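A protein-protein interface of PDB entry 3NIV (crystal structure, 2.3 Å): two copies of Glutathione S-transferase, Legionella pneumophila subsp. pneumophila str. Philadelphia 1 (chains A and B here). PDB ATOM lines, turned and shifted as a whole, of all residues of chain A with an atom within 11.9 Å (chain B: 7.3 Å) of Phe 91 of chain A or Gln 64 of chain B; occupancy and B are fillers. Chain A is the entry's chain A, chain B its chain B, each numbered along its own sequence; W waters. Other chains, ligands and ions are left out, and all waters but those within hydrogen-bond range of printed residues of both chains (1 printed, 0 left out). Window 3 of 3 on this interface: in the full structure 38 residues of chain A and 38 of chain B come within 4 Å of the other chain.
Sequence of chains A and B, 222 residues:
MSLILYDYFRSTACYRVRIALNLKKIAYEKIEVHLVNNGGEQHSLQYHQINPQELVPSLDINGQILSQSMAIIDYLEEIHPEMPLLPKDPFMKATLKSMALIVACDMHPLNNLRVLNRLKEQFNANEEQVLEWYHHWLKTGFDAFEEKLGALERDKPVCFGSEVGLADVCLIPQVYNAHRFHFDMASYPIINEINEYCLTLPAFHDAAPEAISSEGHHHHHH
NZ of Lys 93 of chain A is in salt-bridge range of OE1 of Glu 78 of chain B, 3.3 Å away. The side-chain amino group (NZ) of Lys 148 of chain A sits at hydrogen-bond distance from the side-chain hydroxyl (OG) of Ser 67 of chain B.
The backbone carbonyl oxygen of Phe 91 of chain A sits at hydrogen-bond distance from the side-chain hydroxyl of Thr 95 of chain A. OG of Ser 98 of chain A sits at hydrogen-bond distance from O of Thr 95 of chain A (2.9 Å). The backbone carbonyl oxygen (O) of Leu 59 of chain B sits at hydrogen-bond distance from the backbone NH (N) of Leu 66 of chain B, at 2.7 Å.
Pro 90 of chain A touches Tyr 75 of chain B. Ile 61 of chain B touches Phe 91 of chain A (CD1 to CE1, 3.997 Å). Phe 91 of chain A touches Gln 64 of chain B. Ile 65 of chain B touches Phe 91 of chain A (O to CZ, 3.8 Å). Phe 91 of chain A touches Tyr 75 of chain B (CA to CE1, 3.8 Å). O of Ala 94 of chain A touches CD1 of Leu 66 of chain B (3.5 Å). Ala 94 of chain A touches Tyr 75 of chain B. CA of Thr 95 of chain A touches CD1 of Leu 66 of chain B (3.8 Å).
Printed residues of chain B within 4 Å of Phe 91 of chain A: Ile 61 (3.997 Å), Gln 64 (3.4 Å), Ile 65 (3.8 Å) and Tyr 75 (3.8 Å). Gln 64 of chain B touches one residue of chain A. No residue of chain A comes within 4 Å of Leu 59 of chain B. No residue of chain A comes within 4 Å of Asp 60 of chain B. No residue of chain A comes within 4 Å of Asn 62 of chain B. No residue of chain A comes within 4 Å of Gly 63 of chain B. Ile 65 of chain B touches one residue of chain A. Leu 66 of chain B touches just these residues of chain A: Ala 94 (3.5 Å) and Thr 95 (3.8 Å). Of the printed residues of chain A, Tyr 75 of chain B touches Pro 90, Phe 91 and Ala 94. Of the printed residues of chain A, Ser 67 of chain B touches Lys 148. Of the printed residues of chain A, Glu 78 of chain B touches Lys 93. Of the printed residues of chain A, Ile 61 of chain B touches Phe 91 (3.997 Å). The nearest printed residue of chain B that does not touch Phe 91 of chain A is Leu 66 of chain B (4.2 Å). The nearest printed residue of chain B that does not touch Lys 148 of chain A is Leu 66 of chain B (5.7 Å).
Hydrophobic or aromatic side chains of chain A within 4 Å of the printed part of chain B: Phe 91 and Ala 94. Printed residues of chain B that touch a printed residue of chain A: Ile 61, Gln 64, Ile 65, Leu 66, Ser 67, Tyr 75 and Glu 78. Hydrophobic or aromatic side chains of chain B that line the printed part of chain A: Ile 61, Leu 66 and Tyr 75. Among the printed residues, 10 pairs touch across the chains. Among the printed residues, Asp or Glu carboxylates within 4 Å of a Lys or Arg side-chain nitrogen of the other chain: Lys 93 of chain A with Glu 78 of chain B (3.3 Å).
No position is printed for both chains.
Water W1 lies within hydrogen-bond range of N of Ser 67 of chain B, NZ of Lys 148 of chain A and OG of Ser 98 of chain A.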
ATOM      1  N   LEU A  85     -19.028  -2.624   6.775  1.00  0.00           N
ATOM      2  CA  LEU A  85     -19.597  -2.094   5.545  1.00  0.00           C
ATOM      3  C   LEU A  85     -19.413  -3.089   4.410  1.00  0.00           C
ATOM      4  O   LEU A  85     -19.844  -2.862   3.283  1.00  0.00           O
ATOM      5  CB  LEU A  85     -18.976  -0.743   5.205  1.00  0.00           C
ATOM      6  CG  LEU A  85     -19.222   0.324   6.275  1.00  0.00           C
ATOM      7  CD1 LEU A  85     -18.407   1.578   5.996  1.00  0.00           C
ATOM      8  CD2 LEU A  85     -20.705   0.637   6.372  1.00  0.00           C
ATOM      9  N   LEU A  86     -18.788  -4.215   4.730  1.00  0.00           N
ATOM     10  CA  LEU A  86     -18.547  -5.251   3.740  1.00  0.00           C
ATOM     11  C   LEU A  86     -18.728  -6.643   4.322  1.00  0.00           C
ATOM     12  O   LEU A  86     -18.422  -6.873   5.492  1.00  0.00           O
ATOM     13  CB  LEU A  86     -17.131  -5.109   3.182  1.00  0.00           C
ATOM     14  CG  LEU A  86     -16.951  -3.927   2.234  1.00  0.00           C
ATOM     15  CD1 LEU A  86     -15.500  -3.489   2.192  1.00  0.00           C
ATOM     16  CD2 LEU A  86     -17.464  -4.275   0.843  1.00  0.00           C
ATOM     17  N   PRO A  87     -19.202  -7.582   3.492  1.00  0.00           N
ATOM     18  CA  PRO A  87     -19.330  -9.004   3.838  1.00  0.00           C
ATOM     19  C   PRO A  87     -17.972  -9.633   4.185  1.00  0.00           C
ATOM     20  O   PRO A  87     -16.923  -9.038   3.916  1.00  0.00           O
ATOM     21  CB  PRO A  87     -19.863  -9.634   2.547  1.00  0.00           C
ATOM     22  CG  PRO A  87     -20.385  -8.507   1.726  1.00  0.00           C
ATOM     23  CD  PRO A  87     -19.562  -7.316   2.090  1.00  0.00           C
ATOM     24  N   LYS A  88     -17.990 -10.828   4.769  1.00  0.00           N
ATOM     25  CA  LYS A  88     -16.743 -11.535   5.059  1.00  0.00           C
ATOM     26  C   LYS A  88     -16.172 -12.274   3.843  1.00  0.00           C
ATOM     27  O   LYS A  88     -14.965 -12.255   3.613  1.00  0.00           O
ATOM     28  CB  LYS A  88     -16.913 -12.487   6.244  1.00  0.00           C
ATOM     29  CG  LYS A  88     -16.807 -11.815   7.614  1.00  0.00           C
ATOM     30  CD  LYS A  88     -17.087 -12.813   8.726  1.00  0.00           C
ATOM     31  CE  LYS A  88     -17.461 -12.117  10.025  1.00  0.00           C
ATOM     32  NZ  LYS A  88     -18.049 -13.091  10.997  1.00  0.00           N
ATOM     33  N   ASP A  89     -17.041 -12.913   3.067  1.00  0.00           N
ATOM     34  CA  ASP A  89     -16.610 -13.633   1.870  1.00  0.00           C
ATOM     35  C   ASP A  89     -15.703 -12.772   0.985  1.00  0.00           C
ATOM     36  O   ASP A  89     -16.138 -11.771   0.410  1.00  0.00           O
ATOM     37  CB  ASP A  89     -17.826 -14.124   1.080  1.00  0.00           C
ATOM     38  CG  ASP A  89     -17.447 -14.766  -0.244  1.00  0.00           C
ATOM     39  OD1 ASP A  89     -16.487 -15.570  -0.262  1.00  0.00           O
ATOM     40  OD2 ASP A  89     -18.112 -14.479  -1.267  1.00  0.00           O
ATOM     41  N   PRO A  90     -14.430 -13.165   0.877  1.00  0.00           N
ATOM     42  CA  PRO A  90     -13.429 -12.418   0.118  1.00  0.00           C
ATOM     43  C   PRO A  90     -13.906 -12.030  -1.271  1.00  0.00           C
ATOM     44  O   PRO A  90     -13.600 -10.933  -1.712  1.00  0.00           O
ATOM     45  CB  PRO A  90     -12.272 -13.406   0.028  1.00  0.00           C
ATOM     46  CG  PRO A  90     -12.370 -14.156   1.306  1.00  0.00           C
ATOM     47  CD  PRO A  90     -13.832 -14.322   1.569  1.00  0.00           C
ATOM     48  N   PHE A  91     -14.636 -12.905  -1.950  1.00  0.00           N
ATOM     49  CA  PHE A  91     -15.110 -12.578  -3.287  1.00  0.00           C
ATOM     50  C   PHE A  91     -16.236 -11.528  -3.290  1.00  0.00           C
ATOM     51  O   PHE A  91     -16.208 -10.577  -4.077  1.00  0.00           O
ATOM     52  CB  PHE A  91     -15.570 -13.828  -4.031  1.00  0.00           C
ATOM     53  CG  PHE A  91     -16.201 -13.528  -5.362  1.00  0.00           C
ATOM     54  CD1 PHE A  91     -15.415 -13.254  -6.469  1.00  0.00           C
ATOM     55  CD2 PHE A  91     -17.575 -13.502  -5.502  1.00  0.00           C
ATOM     56  CE1 PHE A  91     -15.989 -12.967  -7.695  1.00  0.00           C
ATOM     57  CE2 PHE A  91     -18.155 -13.222  -6.723  1.00  0.00           C
ATOM     58  CZ  PHE A  91     -17.364 -12.951  -7.820  1.00  0.00           C
ATOM     59  N   MET A  92     -17.229 -11.716  -2.425  1.00  0.00           N
ATOM     60  CA  MET A  92     -18.320 -10.751  -2.291  1.00  0.00           C
ATOM     61  C   MET A  92     -17.811  -9.395  -1.844  1.00  0.00           C
ATOM     62  O   MET A  92     -18.266  -8.356  -2.321  1.00  0.00           O
ATOM     63  CB  MET A  92     -19.380 -11.252  -1.308  1.00  0.00           C
ATOM     64  CG  MET A  92     -20.418 -12.114  -1.972  1.00  0.00           C
ATOM     65  SD  MET A  92     -20.979 -11.360  -3.693  1.00  0.00           S
ATOM     66  CE  MET A  92     -21.675  -9.639  -3.067  1.00  0.00           C
ATOM     67  N   LYS A  93     -16.860  -9.411  -0.922  1.00  0.00           N
ATOM     68  CA  LYS A  93     -16.269  -8.182  -0.446  1.00  0.00           C
ATOM     69  C   LYS A  93     -15.649  -7.427  -1.610  1.00  0.00           C
ATOM     70  O   LYS A  93     -15.855  -6.227  -1.756  1.00  0.00           O
ATOM     71  CB  LYS A  93     -15.224  -8.468   0.629  1.00  0.00           C
ATOM     72  CG  LYS A  93     -14.187  -7.382   0.755  1.00  0.00           C
ATOM     73  CD  LYS A  93     -13.761  -7.169   2.194  1.00  0.00           C
ATOM     74  CE  LYS A  93     -13.193  -8.420   2.800  1.00  0.00           C
ATOM     75  NZ  LYS A  93     -13.024  -8.216   4.263  1.00  0.00           N
ATOM     76  N   ALA A  94     -14.906  -8.136  -2.450  1.00  0.00           N
ATOM     77  CA  ALA A  94     -14.238  -7.501  -3.576  1.00  0.00           C
ATOM     78  C   ALA A  94     -15.255  -7.049  -4.624  1.00  0.00           C
ATOM     79  O   ALA A  94     -15.054  -6.060  -5.330  1.00  0.00           O
ATOM     80  CB  ALA A  94     -13.223  -8.451  -4.194  1.00  0.00           C
ATOM     81  N   THR A  95     -16.345  -7.792  -4.728  1.00  0.00           N
ATOM     82  CA  THR A  95     -17.342  -7.525  -5.745  1.00  0.00           C
ATOM     83  C   THR A  95     -18.094  -6.239  -5.437  1.00  0.00           C
ATOM     84  O   THR A  95     -18.340  -5.416  -6.319  1.00  0.00           O
ATOM     85  CB  THR A  95     -18.331  -8.681  -5.825  1.00  0.00           C
ATOM     86  OG1 THR A  95     -17.668  -9.814  -6.392  1.00  0.00           O
ATOM     87  CG2 THR A  95     -19.533  -8.304  -6.689  1.00  0.00           C
ATOM     88  N   LEU A  96     -18.462  -6.079  -4.173  1.00  0.00           N
ATOM     89  CA  LEU A  96     -19.103  -4.864  -3.720  1.00  0.00           C
ATOM     90  C   LEU A  96     -18.158  -3.663  -3.852  1.00  0.00           C
ATOM     91  O   LEU A  96     -18.551  -2.585  -4.289  1.00  0.00           O
ATOM     92  CB  LEU A  96     -19.581  -5.055  -2.282  1.00  0.00           C
ATOM     93  CG  LEU A  96     -20.861  -5.888  -2.228  1.00  0.00           C
ATOM     94  CD1 LEU A  96     -21.082  -6.493  -0.850  1.00  0.00           C
ATOM     95  CD2 LEU A  96     -22.059  -5.049  -2.665  1.00  0.00           C
ATOM     96  N   LYS A  97     -16.904  -3.874  -3.486  1.00  0.00           N
ATOM     97  CA  LYS A  97     -15.865  -2.854  -3.609  1.00  0.00           C
ATOM     98  C   LYS A  97     -15.787  -2.313  -5.023  1.00  0.00           C
ATOM     99  O   LYS A  97     -15.750  -1.101  -5.242  1.00  0.00           O
ATOM    100  CB  LYS A  97     -14.517  -3.458  -3.256  1.00  0.00           C
ATOM    101  CG  LYS A  97     -13.681  -2.609  -2.331  1.00  0.00           C
ATOM    102  CD  LYS A  97     -13.871  -3.033  -0.877  1.00  0.00           C
ATOM    103  CE  LYS A  97     -12.556  -2.935  -0.105  1.00  0.00           C
ATOM    104  NZ  LYS A  97     -11.970  -1.560  -0.142  1.00  0.00           N
ATOM    105  N   SER A  98     -15.762  -3.218  -5.990  1.00  0.00           N
ATOM    106  CA  SER A  98     -15.624  -2.810  -7.370  1.00  0.00           C
ATOM    107  C   SER A  98     -16.852  -2.009  -7.827  1.00  0.00           C
ATOM    108  O   SER A  98     -16.789  -1.221  -8.781  1.00  0.00           O
ATOM    109  CB  SER A  98     -15.404  -4.017  -8.265  1.00  0.00           C
ATOM    110  OG  SER A  98     -16.606  -4.694  -8.527  1.00  0.00           O
ATOM    111  N   MET A  99     -17.970  -2.207  -7.151  1.00  0.00           N
ATOM    112  CA  MET A  99     -19.166  -1.468  -7.512  1.00  0.00           C
ATOM    113  C   MET A  99     -19.071  -0.058  -6.970  1.00  0.00           C
ATOM    114  O   MET A  99     -19.453   0.889  -7.628  1.00  0.00           O
ATOM    115  CB  MET A  99     -20.406  -2.185  -7.002  1.00  0.00           C
ATOM    116  CG  MET A  99     -20.679  -3.445  -7.789  1.00  0.00           C
ATOM    117  SD  MET A  99     -22.031  -4.555  -6.958  1.00  0.00           S
ATOM    118  CE  MET A  99     -23.561  -3.314  -7.104  1.00  0.00           C
ATOM    119  N   ALA A 100     -18.534   0.064  -5.766  1.00  0.00           N
ATOM    120  CA  ALA A 100     -18.235   1.363  -5.205  1.00  0.00           C
ATOM    121  C   ALA A 100     -17.202   2.096  -6.073  1.00  0.00           C
ATOM    122  O   ALA A 100     -17.238   3.312  -6.186  1.00  0.00           O
ATOM    123  CB  ALA A 100     -17.739   1.215  -3.792  1.00  0.00           C
ATOM    124  N   LEU A 101     -16.298   1.349  -6.699  1.00  0.00           N
ATOM    125  CA  LEU A 101     -15.288   1.951  -7.568  1.00  0.00           C
ATOM    126  C   LEU A 101     -15.888   2.450  -8.879  1.00  0.00           C
ATOM    127  O   LEU A 101     -15.461   3.468  -9.432  1.00  0.00           O
ATOM    128  CB  LEU A 101     -14.165   0.954  -7.853  1.00  0.00           C
ATOM    129  CG  LEU A 101     -13.400   0.519  -6.594  1.00  0.00           C
ATOM    130  CD1 LEU A 101     -12.318  -0.543  -6.892  1.00  0.00           C
ATOM    131  CD2 LEU A 101     -12.814   1.729  -5.878  1.00  0.00           C
ATOM    132  N   LYS A 148     -24.607  -5.121 -12.538  1.00  0.00           N
ATOM    133  CA  LYS A 148     -24.073  -6.045 -11.550  1.00  0.00           C
ATOM    134  C   LYS A 148     -25.081  -6.180 -10.416  1.00  0.00           C
ATOM    135  O   LYS A 148     -25.169  -7.209  -9.750  1.00  0.00           O
ATOM    136  CB  LYS A 148     -22.714  -5.559 -11.053  1.00  0.00           C
ATOM    137  CG  LYS A 148     -21.685  -5.413 -12.177  1.00  0.00           C
ATOM    138  CD  LYS A 148     -20.475  -4.579 -11.749  1.00  0.00           C
ATOM    139  CE  LYS A 148     -19.275  -5.436 -11.366  1.00  0.00           C
ATOM    140  NZ  LYS A 148     -18.518  -5.944 -12.554  1.00  0.00           N
ATOM    141  N   LEU A 149     -25.861  -5.128 -10.228  1.00  0.00           N
ATOM    142  CA  LEU A 149     -26.906  -5.110  -9.222  1.00  0.00           C
ATOM    143  C   LEU A 149     -27.855  -6.278  -9.485  1.00  0.00           C
ATOM    144  O   LEU A 149     -28.269  -6.998  -8.562  1.00  0.00           O
ATOM    145  CB  LEU A 149     -27.659  -3.788  -9.334  1.00  0.00           C
ATOM    146  CG  LEU A 149     -28.075  -3.045  -8.075  1.00  0.00           C
ATOM    147  CD1 LEU A 149     -27.030  -3.095  -6.989  1.00  0.00           C
ATOM    148  CD2 LEU A 149     -28.393  -1.610  -8.454  1.00  0.00           C
ATOM    149  N   ALA A 151     -27.359  -9.126 -10.615  1.00  0.00           N
ATOM    150  CA  ALA A 151     -26.854 -10.484 -10.419  1.00  0.00           C
ATOM    151  C   ALA A 151     -26.812 -10.860  -8.938  1.00  0.00           C
ATOM    152  O   ALA A 151     -26.469 -11.992  -8.585  1.00  0.00           O
ATOM    153  CB  ALA A 151     -25.468 -10.658 -11.065  1.00  0.00           C
ATOM    154  N   LEU A 152     -27.170  -9.910  -8.077  1.00  0.00           N
ATOM    155  CA  LEU A 152     -27.141 -10.146  -6.640  1.00  0.00           C
ATOM    156  C   LEU A 152     -28.538 -10.289  -6.030  1.00  0.00           C
ATOM    157  O   LEU A 152     -29.544  -9.845  -6.595  1.00  0.00           O
ATOM    158  CB  LEU A 152     -26.378  -9.031  -5.928  1.00  0.00           C
ATOM    159  CG  LEU A 152     -25.006  -8.639  -6.482  1.00  0.00           C
ATOM    160  CD1 LEU A 152     -24.451  -7.451  -5.706  1.00  0.00           C
ATOM    161  CD2 LEU A 152     -24.018  -9.805  -6.445  1.00  0.00           C
ATOM    162  N   GLU A 153     -28.580 -10.902  -4.857  1.00  0.00           N
ATOM    163  CA  GLU A 153     -29.819 -11.105  -4.137  1.00  0.00           C
ATOM    164  C   GLU A 153     -29.793 -10.240  -2.897  1.00  0.00           C
ATOM    165  O   GLU A 153     -28.717  -9.936  -2.366  1.00  0.00           O
ATOM    166  CB  GLU A 153     -29.954 -12.576  -3.765  1.00  0.00           C
ATOM    167  CG  GLU A 153     -30.066 -13.500  -4.984  1.00  0.00           C
ATOM    168  CD  GLU A 153     -31.483 -13.543  -5.549  1.00  0.00           C
ATOM    169  OE1 GLU A 153     -32.420 -13.849  -4.770  1.00  0.00           O
ATOM    170  OE2 GLU A 153     -31.664 -13.271  -6.765  1.00  0.00           O
ATOM    171  N   PHE A 160     -26.700  -5.446  -1.684  1.00  0.00           N
ATOM    172  CA  PHE A 160     -26.523  -6.876  -1.519  1.00  0.00           C
ATOM    173  C   PHE A 160     -26.860  -7.329  -0.104  1.00  0.00           C
ATOM    174  O   PHE A 160     -26.387  -6.753   0.868  1.00  0.00           O
ATOM    175  CB  PHE A 160     -25.073  -7.261  -1.826  1.00  0.00           C
ATOM    176  CG  PHE A 160     -24.706  -8.632  -1.347  1.00  0.00           C
ATOM    177  CD1 PHE A 160     -25.047  -9.748  -2.088  1.00  0.00           C
ATOM    178  CD2 PHE A 160     -24.063  -8.806  -0.136  1.00  0.00           C
ATOM    179  CE1 PHE A 160     -24.733 -11.013  -1.639  1.00  0.00           C
ATOM    180  CE2 PHE A 160     -23.749 -10.060   0.316  1.00  0.00           C
ATOM    181  CZ  PHE A 160     -24.077 -11.170  -0.440  1.00  0.00           C
ATOM    182  N   LEU A 166     -20.779  -0.614   1.721  1.00  0.00           N
ATOM    183  CA  LEU A 166     -19.927   0.329   1.009  1.00  0.00           C
ATOM    184  C   LEU A 166     -20.516   0.773  -0.319  1.00  0.00           C
ATOM    185  O   LEU A 166     -20.465   1.942  -0.652  1.00  0.00           O
ATOM    186  CB  LEU A 166     -18.534  -0.279   0.766  1.00  0.00           C
ATOM    187  CG  LEU A 166     -17.547   0.608  -0.005  1.00  0.00           C
ATOM    188  CD1 LEU A 166     -17.279   1.908   0.752  1.00  0.00           C
ATOM    189  CD2 LEU A 166     -16.230  -0.135  -0.311  1.00  0.00           C
ATOM    190  N   ALA A 167     -21.051  -0.162  -1.089  1.00  0.00           N
ATOM    191  CA  ALA A 167     -21.683   0.183  -2.351  1.00  0.00           C
ATOM    192  C   ALA A 167     -22.858   1.145  -2.151  1.00  0.00           C
ATOM    193  O   ALA A 167     -23.049   2.071  -2.945  1.00  0.00           O
ATOM    194  CB  ALA A 167     -22.152  -1.067  -3.071  1.00  0.00           C
ATOM    195  N   ILE B   4      -8.149 -16.945 -14.077  1.00  0.00           N
ATOM    196  CA  ILE B   4      -7.882 -16.314 -15.365  1.00  0.00           C
ATOM    197  C   ILE B   4      -7.931 -14.791 -15.362  1.00  0.00           C
ATOM    198  O   ILE B   4      -8.800 -14.184 -14.745  1.00  0.00           O
ATOM    199  CB  ILE B   4      -8.826 -16.800 -16.473  1.00  0.00           C
ATOM    200  CG1 ILE B   4      -8.829 -18.324 -16.572  1.00  0.00           C
ATOM    201  CG2 ILE B   4      -8.422 -16.178 -17.809  1.00  0.00           C
ATOM    202  CD1 ILE B   4     -10.065 -18.976 -15.972  1.00  0.00           C
ATOM    203  N   LEU B  59     -10.606 -10.497 -13.464  1.00  0.00           N
ATOM    204  CA  LEU B  59     -10.110 -11.726 -12.865  1.00  0.00           C
ATOM    205  C   LEU B  59     -11.240 -12.743 -12.791  1.00  0.00           C
ATOM    206  O   LEU B  59     -12.323 -12.435 -12.286  1.00  0.00           O
ATOM    207  CB  LEU B  59      -9.575 -11.451 -11.465  1.00  0.00           C
ATOM    208  CG  LEU B  59      -8.533 -12.465 -11.013  1.00  0.00           C
ATOM    209  CD1 LEU B  59      -7.328 -12.410 -11.948  1.00  0.00           C
ATOM    210  CD2 LEU B  59      -8.123 -12.199  -9.575  1.00  0.00           C
ATOM    211  N   ASP B  60     -10.988 -13.943 -13.314  1.00  0.00           N
ATOM    212  CA  ASP B  60     -11.979 -15.013 -13.347  1.00  0.00           C
ATOM    213  C   ASP B  60     -11.584 -16.107 -12.364  1.00  0.00           C
ATOM    214  O   ASP B  60     -10.712 -16.928 -12.647  1.00  0.00           O
ATOM    215  CB  ASP B  60     -12.104 -15.582 -14.765  1.00  0.00           C
ATOM    216  CG  ASP B  60     -13.150 -16.695 -14.872  1.00  0.00           C
ATOM    217  OD1 ASP B  60     -13.228 -17.551 -13.959  1.00  0.00           O
ATOM    218  OD2 ASP B  60     -13.888 -16.720 -15.883  1.00  0.00           O
ATOM    219  N   ILE B  61     -12.221 -16.096 -11.200  1.00  0.00           N
ATOM    220  CA  ILE B  61     -11.946 -17.070 -10.164  1.00  0.00           C
ATOM    221  C   ILE B  61     -12.975 -18.189 -10.232  1.00  0.00           C
ATOM    222  O   ILE B  61     -14.129 -18.012  -9.840  1.00  0.00           O
ATOM    223  CB  ILE B  61     -11.977 -16.435  -8.756  1.00  0.00           C
ATOM    224  CG1 ILE B  61     -11.346 -15.037  -8.767  1.00  0.00           C
ATOM    225  CG2 ILE B  61     -11.249 -17.322  -7.757  1.00  0.00           C
ATOM    226  CD1 ILE B  61     -12.325 -13.894  -8.996  1.00  0.00           C
ATOM    227  N   ASN B  62     -12.554 -19.339 -10.745  1.00  0.00           N
ATOM    228  CA  ASN B  62     -13.431 -20.494 -10.848  1.00  0.00           C
ATOM    229  C   ASN B  62     -14.789 -20.108 -11.410  1.00  0.00           C
ATOM    230  O   ASN B  62     -15.810 -20.291 -10.744  1.00  0.00           O
ATOM    231  CB  ASN B  62     -13.629 -21.137  -9.471  1.00  0.00           C
ATOM    232  CG  ASN B  62     -12.369 -21.785  -8.942  1.00  0.00           C
ATOM    233  OD1 ASN B  62     -11.695 -22.530  -9.654  1.00  0.00           O
ATOM    234  ND2 ASN B  62     -12.047 -21.515  -7.679  1.00  0.00           N
ATOM    235  N   GLY B  63     -14.800 -19.560 -12.621  1.00  0.00           N
ATOM    236  CA  GLY B  63     -16.047 -19.165 -13.263  1.00  0.00           C
ATOM    237  C   GLY B  63     -16.665 -17.873 -12.747  1.00  0.00           C
ATOM    238  O   GLY B  63     -17.448 -17.236 -13.450  1.00  0.00           O
ATOM    239  N   GLN B  64     -16.329 -17.488 -11.518  1.00  0.00           N
ATOM    240  CA  GLN B  64     -16.768 -16.204 -10.969  1.00  0.00           C
ATOM    241  C   GLN B  64     -15.837 -15.065 -11.418  1.00  0.00           C
ATOM    242  O   GLN B  64     -14.615 -15.158 -11.260  1.00  0.00           O
ATOM    243  CB  GLN B  64     -16.810 -16.263  -9.439  1.00  0.00           C
ATOM    244  CG  GLN B  64     -18.121 -16.741  -8.821  1.00  0.00           C
ATOM    245  CD  GLN B  64     -17.973 -16.983  -7.323  1.00  0.00           C
ATOM    246  OE1 GLN B  64     -16.993 -17.581  -6.877  1.00  0.00           O
ATOM    247  NE2 GLN B  64     -18.936 -16.506  -6.541  1.00  0.00           N
ATOM    248  N   ILE B  65     -16.406 -13.994 -11.966  1.00  0.00           N
ATOM    249  CA  ILE B  65     -15.586 -12.898 -12.488  1.00  0.00           C
ATOM    250  C   ILE B  65     -15.652 -11.612 -11.659  1.00  0.00           C
ATOM    251  O   ILE B  65     -16.702 -11.230 -11.151  1.00  0.00           O
ATOM    252  CB  ILE B  65     -15.908 -12.596 -13.962  1.00  0.00           C
ATOM    253  CG1 ILE B  65     -17.401 -12.388 -14.136  1.00  0.00           C
ATOM    254  CG2 ILE B  65     -15.461 -13.745 -14.852  1.00  0.00           C
ATOM    255  CD1 ILE B  65     -17.818 -12.317 -15.585  1.00  0.00           C
ATOM    256  N   LEU B  66     -14.505 -10.959 -11.528  1.00  0.00           N
ATOM    257  CA  LEU B  66     -14.366  -9.750 -10.727  1.00  0.00           C
ATOM    258  C   LEU B  66     -13.649  -8.691 -11.573  1.00  0.00           C
ATOM    259  O   LEU B  66     -12.711  -9.023 -12.307  1.00  0.00           O
ATOM    260  CB  LEU B  66     -13.575 -10.074  -9.464  1.00  0.00           C
ATOM    261  CG  LEU B  66     -13.118  -8.897  -8.614  1.00  0.00           C
ATOM    262  CD1 LEU B  66     -14.319  -8.215  -7.966  1.00  0.00           C
ATOM    263  CD2 LEU B  66     -12.123  -9.365  -7.578  1.00  0.00           C
ATOM    264  N   SER B  67     -14.063  -7.425 -11.466  1.00  0.00           N
ATOM    265  CA  SER B  67     -13.757  -6.462 -12.527  1.00  0.00           C
ATOM    266  C   SER B  67     -13.042  -5.150 -12.221  1.00  0.00           C
ATOM    267  O   SER B  67     -12.679  -4.431 -13.155  1.00  0.00           O
ATOM    268  CB  SER B  67     -15.022  -6.103 -13.306  1.00  0.00           C
ATOM    269  OG  SER B  67     -15.640  -4.946 -12.753  1.00  0.00           O
ATOM    270  N   TYR B  75      -8.565  -8.125  -3.532  1.00  0.00           N
ATOM    271  CA  TYR B  75      -8.947  -9.523  -3.487  1.00  0.00           C
ATOM    272  C   TYR B  75      -7.700 -10.402  -3.378  1.00  0.00           C
ATOM    273  O   TYR B  75      -7.657 -11.342  -2.580  1.00  0.00           O
ATOM    274  CB  TYR B  75      -9.732  -9.872  -4.738  1.00  0.00           C
ATOM    275  CG  TYR B  75     -10.053 -11.331  -4.869  1.00  0.00           C
ATOM    276  CD1 TYR B  75     -11.152 -11.882  -4.210  1.00  0.00           C
ATOM    277  CD2 TYR B  75      -9.272 -12.163  -5.656  1.00  0.00           C
ATOM    278  CE1 TYR B  75     -11.462 -13.220  -4.327  1.00  0.00           C
ATOM    279  CE2 TYR B  75      -9.569 -13.509  -5.777  1.00  0.00           C
ATOM    280  CZ  TYR B  75     -10.670 -14.031  -5.112  1.00  0.00           C
ATOM    281  OH  TYR B  75     -10.978 -15.373  -5.235  1.00  0.00           O
ATOM    282  N   GLU B  78      -6.369 -10.123   0.141  1.00  0.00           N
ATOM    283  CA  GLU B  78      -7.075 -10.844   1.185  1.00  0.00           C
ATOM    284  C   GLU B  78      -6.839 -12.336   1.015  1.00  0.00           C
ATOM    285  O   GLU B  78      -6.515 -13.042   1.965  1.00  0.00           O
ATOM    286  CB  GLU B  78      -8.562 -10.516   1.214  1.00  0.00           C
ATOM    287  CG  GLU B  78      -9.305 -11.373   2.216  1.00  0.00           C
ATOM    288  CD  GLU B  78     -10.260 -10.580   3.077  1.00  0.00           C
ATOM    289  OE1 GLU B  78     -10.195  -9.329   3.046  1.00  0.00           O
ATOM    290  OE2 GLU B  78     -11.067 -11.213   3.793  1.00  0.00           O
ATOM    291  N   ILE B  79      -6.974 -12.795  -0.216  1.00  0.00           N
ATOM    292  CA  ILE B  79      -6.805 -14.199  -0.528  1.00  0.00           C
ATOM    293  C   ILE B  79      -5.338 -14.665  -0.367  1.00  0.00           C
ATOM    294  O   ILE B  79      -5.071 -15.808   0.010  1.00  0.00           O
ATOM    295  CB  ILE B  79      -7.337 -14.468  -1.935  1.00  0.00           C
ATOM    296  CG1 ILE B  79      -8.810 -14.863  -1.845  1.00  0.00           C
ATOM    297  CG2 ILE B  79      -6.510 -15.510  -2.656  1.00  0.00           C
ATOM    298  CD1 ILE B  79      -9.308 -15.625  -3.032  1.00  0.00           C
HETATM  299  O   HOH W   1     -16.788  -7.171 -10.388  1.00  0.00           O
